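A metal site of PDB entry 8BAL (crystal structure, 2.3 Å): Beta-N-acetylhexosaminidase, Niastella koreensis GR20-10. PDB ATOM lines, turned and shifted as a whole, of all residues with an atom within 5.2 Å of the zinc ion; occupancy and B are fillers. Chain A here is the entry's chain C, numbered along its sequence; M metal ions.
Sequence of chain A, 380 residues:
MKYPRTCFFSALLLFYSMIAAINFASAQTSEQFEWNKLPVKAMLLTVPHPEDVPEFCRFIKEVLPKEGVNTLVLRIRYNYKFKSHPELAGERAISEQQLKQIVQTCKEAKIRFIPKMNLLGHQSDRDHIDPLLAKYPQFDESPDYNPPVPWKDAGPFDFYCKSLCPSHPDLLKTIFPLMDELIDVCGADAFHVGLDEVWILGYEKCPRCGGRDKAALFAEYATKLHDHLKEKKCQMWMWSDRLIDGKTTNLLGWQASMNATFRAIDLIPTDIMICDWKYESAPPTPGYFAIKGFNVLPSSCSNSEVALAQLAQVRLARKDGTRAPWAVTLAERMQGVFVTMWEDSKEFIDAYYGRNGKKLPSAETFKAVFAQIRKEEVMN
The side-chain sulfur (SG) of Cys 206 sits close to the backbone NH (N) of Arg 208, at 3.7 Å.
Cys 165 touches the zinc ion.
The zinc ion is bound by SG of Cys 206 (2.0 Å). The side-chain carboxylate (OE2) of Glu 141 is bound to the zinc ion, 2.2 Å away. SG of Cys 209 is bound to the zinc ion (2.7 Å).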
ATOM      1  N   GLU A 141     -17.597   0.894 -23.173  1.00  0.00           N
ATOM      2  CA  GLU A 141     -17.680   2.145 -23.908  1.00  0.00           C
ATOM      3  C   GLU A 141     -16.285   2.763 -24.056  1.00  0.00           C
ATOM      4  O   GLU A 141     -16.078   3.555 -24.968  1.00  0.00           O
ATOM      5  CB  GLU A 141     -18.701   3.062 -23.203  1.00  0.00           C
ATOM      6  CG  GLU A 141     -19.109   4.311 -23.993  1.00  0.00           C
ATOM      7  CD  GLU A 141     -19.613   4.049 -25.403  1.00  0.00           C
ATOM      8  OE1 GLU A 141     -20.252   4.958 -26.001  1.00  0.00           O
ATOM      9  OE2 GLU A 141     -19.393   2.929 -25.894  1.00  0.00           O
ATOM     10  N   CYS A 165     -21.256  -0.554 -24.138  1.00  0.00           N
ATOM     11  CA  CYS A 165     -21.351  -0.019 -25.484  1.00  0.00           C
ATOM     12  C   CYS A 165     -22.649  -0.520 -26.075  1.00  0.00           C
ATOM     13  O   CYS A 165     -22.679  -1.549 -26.732  1.00  0.00           O
ATOM     14  CB  CYS A 165     -20.127  -0.432 -26.289  1.00  0.00           C
ATOM     15  SG  CYS A 165     -20.567  -1.055 -27.919  1.00  0.00           S
ATOM     16  N   PRO A 166     -23.790   0.176 -25.835  1.00  0.00           N
ATOM     17  CA  PRO A 166     -25.102  -0.375 -26.169  1.00  0.00           C
ATOM     18  C   PRO A 166     -25.480  -0.273 -27.645  1.00  0.00           C
ATOM     19  O   PRO A 166     -26.628  -0.585 -28.030  1.00  0.00           O
ATOM     20  CB  PRO A 166     -26.068   0.416 -25.280  1.00  0.00           C
ATOM     21  CG  PRO A 166     -25.330   1.698 -24.876  1.00  0.00           C
ATOM     22  CD  PRO A 166     -23.874   1.534 -25.281  1.00  0.00           C
ATOM     23  N   SER A 167     -24.512   0.182 -28.457  1.00  0.00           N
ATOM     24  CA  SER A 167     -24.545  -0.062 -29.893  1.00  0.00           C
ATOM     25  C   SER A 167     -23.941  -1.419 -30.227  1.00  0.00           C
ATOM     26  O   SER A 167     -23.828  -1.749 -31.410  1.00  0.00           O
ATOM     27  CB  SER A 167     -23.866   1.047 -30.666  1.00  0.00           C
ATOM     28  OG  SER A 167     -24.763   2.116 -30.902  1.00  0.00           O
ATOM     29  N   CYS A 206     -15.373   4.940 -29.714  1.00  0.00           N
ATOM     30  CA  CYS A 206     -16.193   3.758 -29.956  1.00  0.00           C
ATOM     31  C   CYS A 206     -16.463   3.695 -31.461  1.00  0.00           C
ATOM     32  O   CYS A 206     -17.033   4.637 -32.012  1.00  0.00           O
ATOM     33  CB  CYS A 206     -17.503   3.809 -29.169  1.00  0.00           C
ATOM     34  SG  CYS A 206     -18.461   2.259 -29.127  1.00  0.00           S
ATOM     35  N   ARG A 208     -18.661   2.242 -32.780  1.00  0.00           N
ATOM     36  CA  ARG A 208     -20.119   2.168 -32.808  1.00  0.00           C
ATOM     37  C   ARG A 208     -20.738   3.489 -32.358  1.00  0.00           C
ATOM     38  O   ARG A 208     -21.415   4.135 -33.153  1.00  0.00           O
ATOM     39  CB  ARG A 208     -20.535   0.981 -31.944  1.00  0.00           C
ATOM     40  CG  ARG A 208     -20.087  -0.351 -32.526  1.00  0.00           C
ATOM     41  CD  ARG A 208     -20.173  -1.532 -31.584  1.00  0.00           C
ATOM     42  NE  ARG A 208     -19.025  -2.402 -31.835  1.00  0.00           N
ATOM     43  CZ  ARG A 208     -17.770  -2.071 -31.564  1.00  0.00           C
ATOM     44  NH1 ARG A 208     -17.489  -1.226 -30.575  1.00  0.00           N
ATOM     45  NH2 ARG A 208     -16.790  -2.617 -32.275  1.00  0.00           N
ATOM     46  N   CYS A 209     -20.451   3.917 -31.115  1.00  0.00           N
ATOM     47  CA  CYS A 209     -21.104   5.055 -30.473  1.00  0.00           C
ATOM     48  C   CYS A 209     -20.401   6.397 -30.752  1.00  0.00           C
ATOM     49  O   CYS A 209     -21.011   7.457 -30.577  1.00  0.00           O
ATOM     50  CB  CYS A 209     -21.157   4.874 -28.955  1.00  0.00           C
ATOM     51  SG  CYS A 209     -22.318   3.613 -28.359  1.00  0.00           S
HETATM   52 ZN    ZN M   1     -20.008   2.276 -27.912  1.00  0.00          ZN
